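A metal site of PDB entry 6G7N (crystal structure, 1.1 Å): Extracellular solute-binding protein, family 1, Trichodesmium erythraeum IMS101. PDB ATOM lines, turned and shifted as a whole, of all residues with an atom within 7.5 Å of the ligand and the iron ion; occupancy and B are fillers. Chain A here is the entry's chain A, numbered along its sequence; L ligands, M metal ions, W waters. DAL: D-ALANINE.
An oxygen (OXT) of the ligand lies within hydrogen-bond range of the side-chain hydroxyl (OH) of Tyr 11. The guanidinium group of Arg 101 lies within salt-bridge range of an oxygen (OXT) of the ligand (3.9 Å). An oxygen (OXT) of the ligand lies within hydrogen-bond range of the side-chain amide nitrogen of Asn 268, 3.3 Å away.
The side-chain amide oxygen of Asn 139 sits at hydrogen-bond distance from the backbone NH of Tyr 141 (3.0 Å). OH of Tyr 197 sits close to NH2 of Arg 101 (3.1 Å). OH of Tyr 197 sits close to ND2 of Asn 195, at 3.0 Å. OH of Tyr 11 sits at hydrogen-bond distance from OD1 of Asn 268 (3.5 Å). The guanidinium group (NH2) of Arg 101 lies close to the side-chain amide nitrogen (ND2) of Asn 195 (3.5 Å). OE2 of Glu 270 lies within salt-bridge range of NH1 of Arg 101 (2.9 Å). The side-chain amide nitrogen (ND2) of Asn 268 sits at hydrogen-bond distance from the side-chain carboxylate (OE2) of Glu 270 (2.8 Å). O of Val 58 lies within hydrogen-bond range of NH2 of Arg 62 (3.0 Å).
Residues that only touch the ligand: Arg 9 (3.9 Å) and Val 58 (3.95 Å).
Of the 22 residues printed, 3 come within 4 Å of the iron ion. The nearest printed residue that does not touch the iron ion is Arg 101 (4.2 Å).
The iron ion is bound by the side-chain hydroxyl (OH) of Tyr 141 (2.0 Å), the side-chain hydroxyl (OH) of Tyr 197 (2.0 Å), the side-chain hydroxyl (OH) of Tyr 198 (2.0 Å), an oxygen (O) of the ligand (2.1 Å) and a nitrogen (N) of the ligand (2.2 Å). The iron ion has five donor atoms within binding distance.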
ATOM      1  N   SER A   8      -8.649 -20.669  31.513  1.00  0.00           N
ATOM      2  CA  SER A   8      -9.649 -21.608  30.980  1.00  0.00           C
ATOM      3  C   SER A   8     -10.554 -21.009  29.890  1.00  0.00           C
ATOM      4  O   SER A   8     -11.481 -21.668  29.405  1.00  0.00           O
ATOM      5  CB  SER A   8     -10.505 -22.149  32.142  1.00  0.00           C
ATOM      6  OG  SER A   8     -11.301 -21.123  32.706  1.00  0.00           O
ATOM      7  N   ARG A   9     -10.312 -19.740  29.558  1.00  0.00           N
ATOM      8  CA  ARG A   9     -11.236 -18.876  28.787  1.00  0.00           C
ATOM      9  C   ARG A   9     -10.658 -18.459  27.425  1.00  0.00           C
ATOM     10  O   ARG A   9     -11.240 -17.640  26.706  1.00  0.00           O
ATOM     11  CB  ARG A   9     -11.583 -17.651  29.682  1.00  0.00           C
ATOM     12  CG  ARG A   9     -12.438 -16.487  29.114  1.00  0.00           C
ATOM     13  CD  ARG A   9     -13.758 -16.881  28.473  1.00  0.00           C
ATOM     14  NE  ARG A   9     -14.468 -15.713  27.967  1.00  0.00           N
ATOM     15  CZ  ARG A   9     -14.141 -15.077  26.849  1.00  0.00           C
ATOM     16  NH1 ARG A   9     -13.155 -15.500  26.078  1.00  0.00           N
ATOM     17  NH2 ARG A   9     -14.830 -13.989  26.484  1.00  0.00           N
ATOM     18  N   HIS A  10      -9.535 -19.059  27.033  1.00  0.00           N
ATOM     19  CA  HIS A  10      -8.911 -18.720  25.759  1.00  0.00           C
ATOM     20  C   HIS A  10      -9.745 -19.270  24.596  1.00  0.00           C
ATOM     21  O   HIS A  10     -10.120 -20.439  24.573  1.00  0.00           O
ATOM     22  CB  HIS A  10      -7.482 -19.302  25.691  1.00  0.00           C
ATOM     23  CG  HIS A  10      -6.839 -19.184  24.348  1.00  0.00           C
ATOM     24  ND1 HIS A  10      -6.175 -18.056  23.917  1.00  0.00           N
ATOM     25  CD2 HIS A  10      -6.783 -20.079  23.326  1.00  0.00           C
ATOM     26  CE1 HIS A  10      -5.725 -18.274  22.694  1.00  0.00           C
ATOM     27  NE2 HIS A  10      -6.085 -19.490  22.317  1.00  0.00           N
ATOM     28  N   TYR A  11      -9.960 -18.425  23.585  1.00  0.00           N
ATOM     29  CA  TYR A  11     -10.439 -18.817  22.253  1.00  0.00           C
ATOM     30  C   TYR A  11      -9.365 -18.431  21.235  1.00  0.00           C
ATOM     31  O   TYR A  11      -8.582 -17.513  21.475  1.00  0.00           O
ATOM     32  CB  TYR A  11     -11.788 -18.164  21.929  1.00  0.00           C
ATOM     33  CG  TYR A  11     -12.886 -18.774  22.752  1.00  0.00           C
ATOM     34  CD1 TYR A  11     -13.476 -19.979  22.389  1.00  0.00           C
ATOM     35  CD2 TYR A  11     -13.284 -18.194  23.949  1.00  0.00           C
ATOM     36  CE1 TYR A  11     -14.477 -20.537  23.186  1.00  0.00           C
ATOM     37  CE2 TYR A  11     -14.256 -18.754  24.752  1.00  0.00           C
ATOM     38  CZ  TYR A  11     -14.860 -19.918  24.366  1.00  0.00           C
ATOM     39  OH  TYR A  11     -15.841 -20.467  25.168  1.00  0.00           O
ATOM     40  N   LYS A  35      -8.960 -26.543  32.672  1.00  0.00           N
ATOM     41  CA  LYS A  35     -10.282 -26.210  33.181  1.00  0.00           C
ATOM     42  C   LYS A  35     -10.081 -25.319  34.419  1.00  0.00           C
ATOM     43  O   LYS A  35      -9.058 -25.403  35.102  1.00  0.00           O
ATOM     44  CB  LYS A  35     -11.068 -27.483  33.493  1.00  0.00           C
ATOM     45  CG  LYS A  35     -11.236 -28.405  32.282  1.00  0.00           C
ATOM     46  CD  LYS A  35     -12.106 -27.828  31.158  1.00  0.00           C
ATOM     47  CE  LYS A  35     -12.259 -28.789  29.983  1.00  0.00           C
ATOM     48  NZ  LYS A  35     -13.479 -28.515  29.147  1.00  0.00           N
ATOM     49  N   THR A  57     -10.632 -17.027  34.089  1.00  0.00           N
ATOM     50  CA  THR A  57     -11.635 -18.088  34.027  1.00  0.00           C
ATOM     51  C   THR A  57     -12.995 -17.459  33.840  1.00  0.00           C
ATOM     52  O   THR A  57     -13.115 -16.257  33.635  1.00  0.00           O
ATOM     53  CB  THR A  57     -11.546 -19.014  35.261  1.00  0.00           C
ATOM     54  OG1 THR A  57     -12.289 -20.215  35.039  1.00  0.00           O
ATOM     55  CG2 THR A  57     -12.069 -18.341  36.533  1.00  0.00           C
ATOM     56  N   VAL A  58     -14.039 -18.292  33.838  1.00  0.00           N
ATOM     57  CA  VAL A  58     -15.418 -17.788  33.797  1.00  0.00           C
ATOM     58  C   VAL A  58     -16.138 -18.062  35.114  1.00  0.00           C
ATOM     59  O   VAL A  58     -15.886 -19.071  35.789  1.00  0.00           O
ATOM     60  CB  VAL A  58     -16.293 -18.264  32.606  1.00  0.00           C
ATOM     61  CG1 VAL A  58     -15.506 -18.145  31.312  1.00  0.00           C
ATOM     62  CG2 VAL A  58     -16.779 -19.687  32.779  1.00  0.00           C
ATOM     63  N   ASP A  59     -17.030 -17.117  35.405  1.00  0.00           N
ATOM     64  CA  ASP A  59     -17.970 -17.105  36.527  1.00  0.00           C
ATOM     65  C   ASP A  59     -17.357 -16.516  37.777  1.00  0.00           C
ATOM     66  O   ASP A  59     -16.328 -17.005  38.260  1.00  0.00           O
ATOM     67  CB  ASP A  59     -18.672 -18.468  36.767  1.00  0.00           C
ATOM     68  CG  ASP A  59     -20.036 -18.297  37.367  1.00  0.00           C
ATOM     69  OD1 ASP A  59     -20.108 -17.837  38.525  1.00  0.00           O
ATOM     70  OD2 ASP A  59     -21.022 -18.556  36.650  1.00  0.00           O
ATOM     71  N   ARG A  62     -16.270 -19.026  40.390  1.00  0.00           N
ATOM     72  CA  ARG A  62     -14.921 -19.640  40.269  1.00  0.00           C
ATOM     73  C   ARG A  62     -13.837 -18.648  40.683  1.00  0.00           C
ATOM     74  O   ARG A  62     -12.852 -19.039  41.307  1.00  0.00           O
ATOM     75  CB  ARG A  62     -14.601 -20.145  38.850  1.00  0.00           C
ATOM     76  CG  ARG A  62     -15.435 -21.294  38.287  1.00  0.00           C
ATOM     77  CD  ARG A  62     -14.739 -22.015  37.124  1.00  0.00           C
ATOM     78  NE  ARG A  62     -15.506 -23.114  36.516  1.00  0.00           N
ATOM     79  CZ  ARG A  62     -16.320 -23.011  35.474  1.00  0.00           C
ATOM     80  NH1 ARG A  62     -16.955 -24.086  34.997  1.00  0.00           N
ATOM     81  NH2 ARG A  62     -16.516 -21.837  34.880  1.00  0.00           N
ATOM     82  N   ARG A 101     -21.808 -11.893  30.637  1.00  0.00           N
ATOM     83  CA  ARG A 101     -22.862 -12.789  30.134  1.00  0.00           C
ATOM     84  C   ARG A 101     -24.104 -12.575  30.985  1.00  0.00           C
ATOM     85  O   ARG A 101     -24.042 -12.125  32.114  1.00  0.00           O
ATOM     86  CB  ARG A 101     -22.419 -14.255  30.130  1.00  0.00           C
ATOM     87  CG  ARG A 101     -21.981 -14.829  31.486  1.00  0.00           C
ATOM     88  CD  ARG A 101     -20.488 -14.716  31.802  1.00  0.00           C
ATOM     89  NE  ARG A 101     -19.613 -15.354  30.832  1.00  0.00           N
ATOM     90  CZ  ARG A 101     -19.481 -16.682  30.673  1.00  0.00           C
ATOM     91  NH1 ARG A 101     -18.720 -17.136  29.699  1.00  0.00           N
ATOM     92  NH2 ARG A 101     -20.110 -17.550  31.464  1.00  0.00           N
ATOM     93  N   ARG A 103     -27.732 -14.616  32.384  1.00  0.00           N
ATOM     94  CA  ARG A 103     -28.442 -15.887  32.480  1.00  0.00           C
ATOM     95  C   ARG A 103     -29.923 -15.562  32.290  1.00  0.00           C
ATOM     96  O   ARG A 103     -30.541 -14.894  33.119  1.00  0.00           O
ATOM     97  CB  ARG A 103     -28.120 -16.647  33.770  1.00  0.00           C
ATOM     98  CG  ARG A 103     -28.543 -18.118  33.724  1.00  0.00           C
ATOM     99  CD  ARG A 103     -27.648 -19.000  34.581  1.00  0.00           C
ATOM    100  NE  ARG A 103     -27.853 -20.431  34.374  1.00  0.00           N
ATOM    101  CZ  ARG A 103     -27.400 -21.103  33.303  1.00  0.00           C
ATOM    102  NH1 ARG A 103     -26.724 -20.507  32.337  1.00  0.00           N
ATOM    103  NH2 ARG A 103     -27.634 -22.417  33.209  1.00  0.00           N
ATOM    104  N   ARG A 135     -30.130 -27.325  33.078  1.00  0.00           N
ATOM    105  CA  ARG A 135     -29.066 -28.297  33.370  1.00  0.00           C
ATOM    106  C   ARG A 135     -28.910 -28.536  34.866  1.00  0.00           C
ATOM    107  O   ARG A 135     -29.606 -27.914  35.711  1.00  0.00           O
ATOM    108  CB  ARG A 135     -27.755 -27.840  32.734  1.00  0.00           C
ATOM    109  CG  ARG A 135     -27.096 -26.680  33.429  1.00  0.00           C
ATOM    110  CD  ARG A 135     -25.990 -26.108  32.621  1.00  0.00           C
ATOM    111  NE  ARG A 135     -24.856 -26.995  32.432  1.00  0.00           N
ATOM    112  CZ  ARG A 135     -23.794 -26.669  31.689  1.00  0.00           C
ATOM    113  NH1 ARG A 135     -23.757 -25.487  31.050  1.00  0.00           N
ATOM    114  NH2 ARG A 135     -22.793 -27.519  31.566  1.00  0.00           N
ATOM    115  N   ASN A 139     -23.568 -27.322  37.822  1.00  0.00           N
ATOM    116  CA  ASN A 139     -23.079 -26.255  36.974  1.00  0.00           C
ATOM    117  C   ASN A 139     -22.971 -24.922  37.726  1.00  0.00           C
ATOM    118  O   ASN A 139     -23.896 -24.491  38.397  1.00  0.00           O
ATOM    119  CB  ASN A 139     -24.034 -26.119  35.796  1.00  0.00           C
ATOM    120  CG  ASN A 139     -23.782 -24.862  35.000  1.00  0.00           C
ATOM    121  OD1 ASN A 139     -24.544 -23.892  35.103  1.00  0.00           O
ATOM    122  ND2 ASN A 139     -22.712 -24.846  34.219  1.00  0.00           N
ATOM    123  N   TYR A 141     -22.955 -21.850  36.647  1.00  0.00           N
ATOM    124  CA  TYR A 141     -23.869 -20.782  36.265  1.00  0.00           C
ATOM    125  C   TYR A 141     -25.155 -20.825  37.097  1.00  0.00           C
ATOM    126  O   TYR A 141     -25.678 -19.801  37.533  1.00  0.00           O
ATOM    127  CB  TYR A 141     -24.225 -20.808  34.784  1.00  0.00           C
ATOM    128  CG  TYR A 141     -23.088 -21.031  33.805  1.00  0.00           C
ATOM    129  CD1 TYR A 141     -21.829 -20.441  34.014  1.00  0.00           C
ATOM    130  CD2 TYR A 141     -23.268 -21.774  32.662  1.00  0.00           C
ATOM    131  CE1 TYR A 141     -20.803 -20.635  33.108  1.00  0.00           C
ATOM    132  CE2 TYR A 141     -22.240 -21.960  31.733  1.00  0.00           C
ATOM    133  CZ  TYR A 141     -21.014 -21.379  31.947  1.00  0.00           C
ATOM    134  OH  TYR A 141     -19.989 -21.579  31.064  1.00  0.00           O
ATOM    135  N   ASP A 177     -25.867 -26.073  28.500  1.00  0.00           N
ATOM    136  CA  ASP A 177     -26.798 -24.985  28.217  1.00  0.00           C
ATOM    137  C   ASP A 177     -27.350 -25.077  26.793  1.00  0.00           C
ATOM    138  O   ASP A 177     -28.518 -24.857  26.555  1.00  0.00           O
ATOM    139  CB  ASP A 177     -26.160 -23.586  28.409  1.00  0.00           C
ATOM    140  CG  ASP A 177     -26.301 -23.011  29.822  1.00  0.00           C
ATOM    141  OD1 ASP A 177     -26.674 -23.752  30.778  1.00  0.00           O
ATOM    142  OD2 ASP A 177     -26.043 -21.793  29.958  1.00  0.00           O
ATOM    143  N   ASN A 195     -27.138 -19.248  29.350  1.00  0.00           N
ATOM    144  CA  ASN A 195     -26.415 -17.993  29.148  1.00  0.00           C
ATOM    145  C   ASN A 195     -26.666 -17.456  27.729  1.00  0.00           C
ATOM    146  O   ASN A 195     -26.726 -18.225  26.766  1.00  0.00           O
ATOM    147  CB  ASN A 195     -24.912 -18.163  29.410  1.00  0.00           C
ATOM    148  CG  ASN A 195     -24.553 -18.354  30.874  1.00  0.00           C
ATOM    149  OD1 ASN A 195     -25.354 -18.050  31.776  1.00  0.00           O
ATOM    150  ND2 ASN A 195     -23.344 -18.830  31.117  1.00  0.00           N
ATOM    151  N   TYR A 197     -24.841 -15.967  25.502  1.00  0.00           N
ATOM    152  CA  TYR A 197     -23.911 -16.226  24.422  1.00  0.00           C
ATOM    153  C   TYR A 197     -24.132 -17.560  23.743  1.00  0.00           C
ATOM    154  O   TYR A 197     -23.661 -17.744  22.611  1.00  0.00           O
ATOM    155  CB  TYR A 197     -22.453 -16.049  24.907  1.00  0.00           C
ATOM    156  CG  TYR A 197     -22.055 -16.953  26.028  1.00  0.00           C
ATOM    157  CD1 TYR A 197     -21.599 -18.243  25.816  1.00  0.00           C
ATOM    158  CD2 TYR A 197     -22.135 -16.527  27.354  1.00  0.00           C
ATOM    159  CE1 TYR A 197     -21.241 -19.066  26.885  1.00  0.00           C
ATOM    160  CE2 TYR A 197     -21.793 -17.346  28.424  1.00  0.00           C
ATOM    161  CZ  TYR A 197     -21.378 -18.634  28.214  1.00  0.00           C
ATOM    162  OH  TYR A 197     -21.104 -19.459  29.260  1.00  0.00           O
ATOM    163  N   TYR A 198     -24.821 -18.515  24.376  1.00  0.00           N
ATOM    164  CA  TYR A 198     -25.064 -19.798  23.723  1.00  0.00           C
ATOM    165  C   TYR A 198     -26.096 -19.662  22.608  1.00  0.00           C
ATOM    166  O   TYR A 198     -26.019 -20.385  21.603  1.00  0.00           O
ATOM    167  CB  TYR A 198     -25.480 -20.888  24.731  1.00  0.00           C
ATOM    168  CG  TYR A 198     -24.368 -21.307  25.658  1.00  0.00           C
ATOM    169  CD1 TYR A 198     -23.229 -21.934  25.191  1.00  0.00           C
ATOM    170  CD2 TYR A 198     -24.450 -21.029  27.018  1.00  0.00           C
ATOM    171  CE1 TYR A 198     -22.223 -22.296  26.047  1.00  0.00           C
ATOM    172  CE2 TYR A 198     -23.431 -21.389  27.879  1.00  0.00           C
ATOM    173  CZ  TYR A 198     -22.309 -22.014  27.398  1.00  0.00           C
ATOM    174  OH  TYR A 198     -21.278 -22.347  28.238  1.00  0.00           O
ATOM    175  N   ARG A 201     -24.204 -17.959  19.784  1.00  0.00           N
ATOM    176  CA  ARG A 201     -23.313 -18.916  19.139  1.00  0.00           C
ATOM    177  C   ARG A 201     -24.041 -19.703  18.038  1.00  0.00           C
ATOM    178  O   ARG A 201     -23.504 -19.892  16.939  1.00  0.00           O
ATOM    179  CB  ARG A 201     -22.735 -19.856  20.177  1.00  0.00           C
ATOM    180  CG  ARG A 201     -21.677 -20.771  19.650  1.00  0.00           C
ATOM    181  CD  ARG A 201     -21.173 -21.700  20.740  1.00  0.00           C
ATOM    182  NE  ARG A 201     -20.502 -21.017  21.855  1.00  0.00           N
ATOM    183  CZ  ARG A 201     -19.992 -21.665  22.896  1.00  0.00           C
ATOM    184  NH1 ARG A 201     -20.147 -22.983  22.994  1.00  0.00           N
ATOM    185  NH2 ARG A 201     -19.339 -21.025  23.848  1.00  0.00           N
ATOM    186  N   SER A 234     -16.727 -13.215  32.593  1.00  0.00           N
ATOM    187  CA  SER A 234     -15.439 -13.803  32.318  1.00  0.00           C
ATOM    188  C   SER A 234     -14.405 -12.854  32.912  1.00  0.00           C
ATOM    189  O   SER A 234     -14.506 -11.647  32.697  1.00  0.00           O
ATOM    190  CB  SER A 234     -15.180 -13.896  30.802  1.00  0.00           C
ATOM    191  OG  SER A 234     -16.080 -14.742  30.132  1.00  0.00           O
ATOM    192  N   ASN A 268     -16.339 -14.867  22.332  1.00  0.00           N
ATOM    193  CA  ASN A 268     -17.360 -15.764  22.837  1.00  0.00           C
ATOM    194  C   ASN A 268     -18.760 -15.182  22.809  1.00  0.00           C
ATOM    195  O   ASN A 268     -19.607 -15.626  23.599  1.00  0.00           O
ATOM    196  CB  ASN A 268     -17.006 -16.271  24.242  1.00  0.00           C
ATOM    197  CG  ASN A 268     -17.880 -17.450  24.670  1.00  0.00           C
ATOM    198  OD1 ASN A 268     -18.211 -18.328  23.844  1.00  0.00           O
ATOM    199  ND2 ASN A 268     -18.208 -17.500  25.968  1.00  0.00           N
ATOM    200  N   GLU A 270     -19.967 -12.543  23.981  1.00  0.00           N
ATOM    201  CA  GLU A 270     -20.279 -11.886  25.249  1.00  0.00           C
ATOM    202  C   GLU A 270     -20.370 -10.365  25.050  1.00  0.00           C
ATOM    203  O   GLU A 270     -20.006  -9.839  23.984  1.00  0.00           O
ATOM    204  CB  GLU A 270     -19.258 -12.292  26.332  1.00  0.00           C
ATOM    205  CG  GLU A 270     -19.408 -13.737  26.712  1.00  0.00           C
ATOM    206  CD  GLU A 270     -18.472 -14.195  27.812  1.00  0.00           C
ATOM    207  OE1 GLU A 270     -18.361 -13.507  28.869  1.00  0.00           O
ATOM    208  OE2 GLU A 270     -17.854 -15.279  27.658  1.00  0.00           O
HETATM  209  N   DAL L   1     -18.292 -22.522  28.909  1.00  0.00           N
HETATM  210  CA  DAL L   1     -17.223 -21.795  28.148  1.00  0.00           C
HETATM  211  CB  DAL L   1     -15.841 -22.278  28.584  1.00  0.00           C
HETATM  212  C   DAL L   1     -17.344 -20.309  28.235  1.00  0.00           C
HETATM  213  O   DAL L   1     -18.370 -19.871  28.795  1.00  0.00           O
HETATM  214  OXT DAL L   1     -16.405 -19.611  27.752  1.00  0.00           O
HETATM  215 FE    FE M   1     -20.008 -21.120  29.160  1.00  0.00          FE
HETATM  216  O   HOH W   1     -18.602 -23.636  25.585  1.00  0.00           O
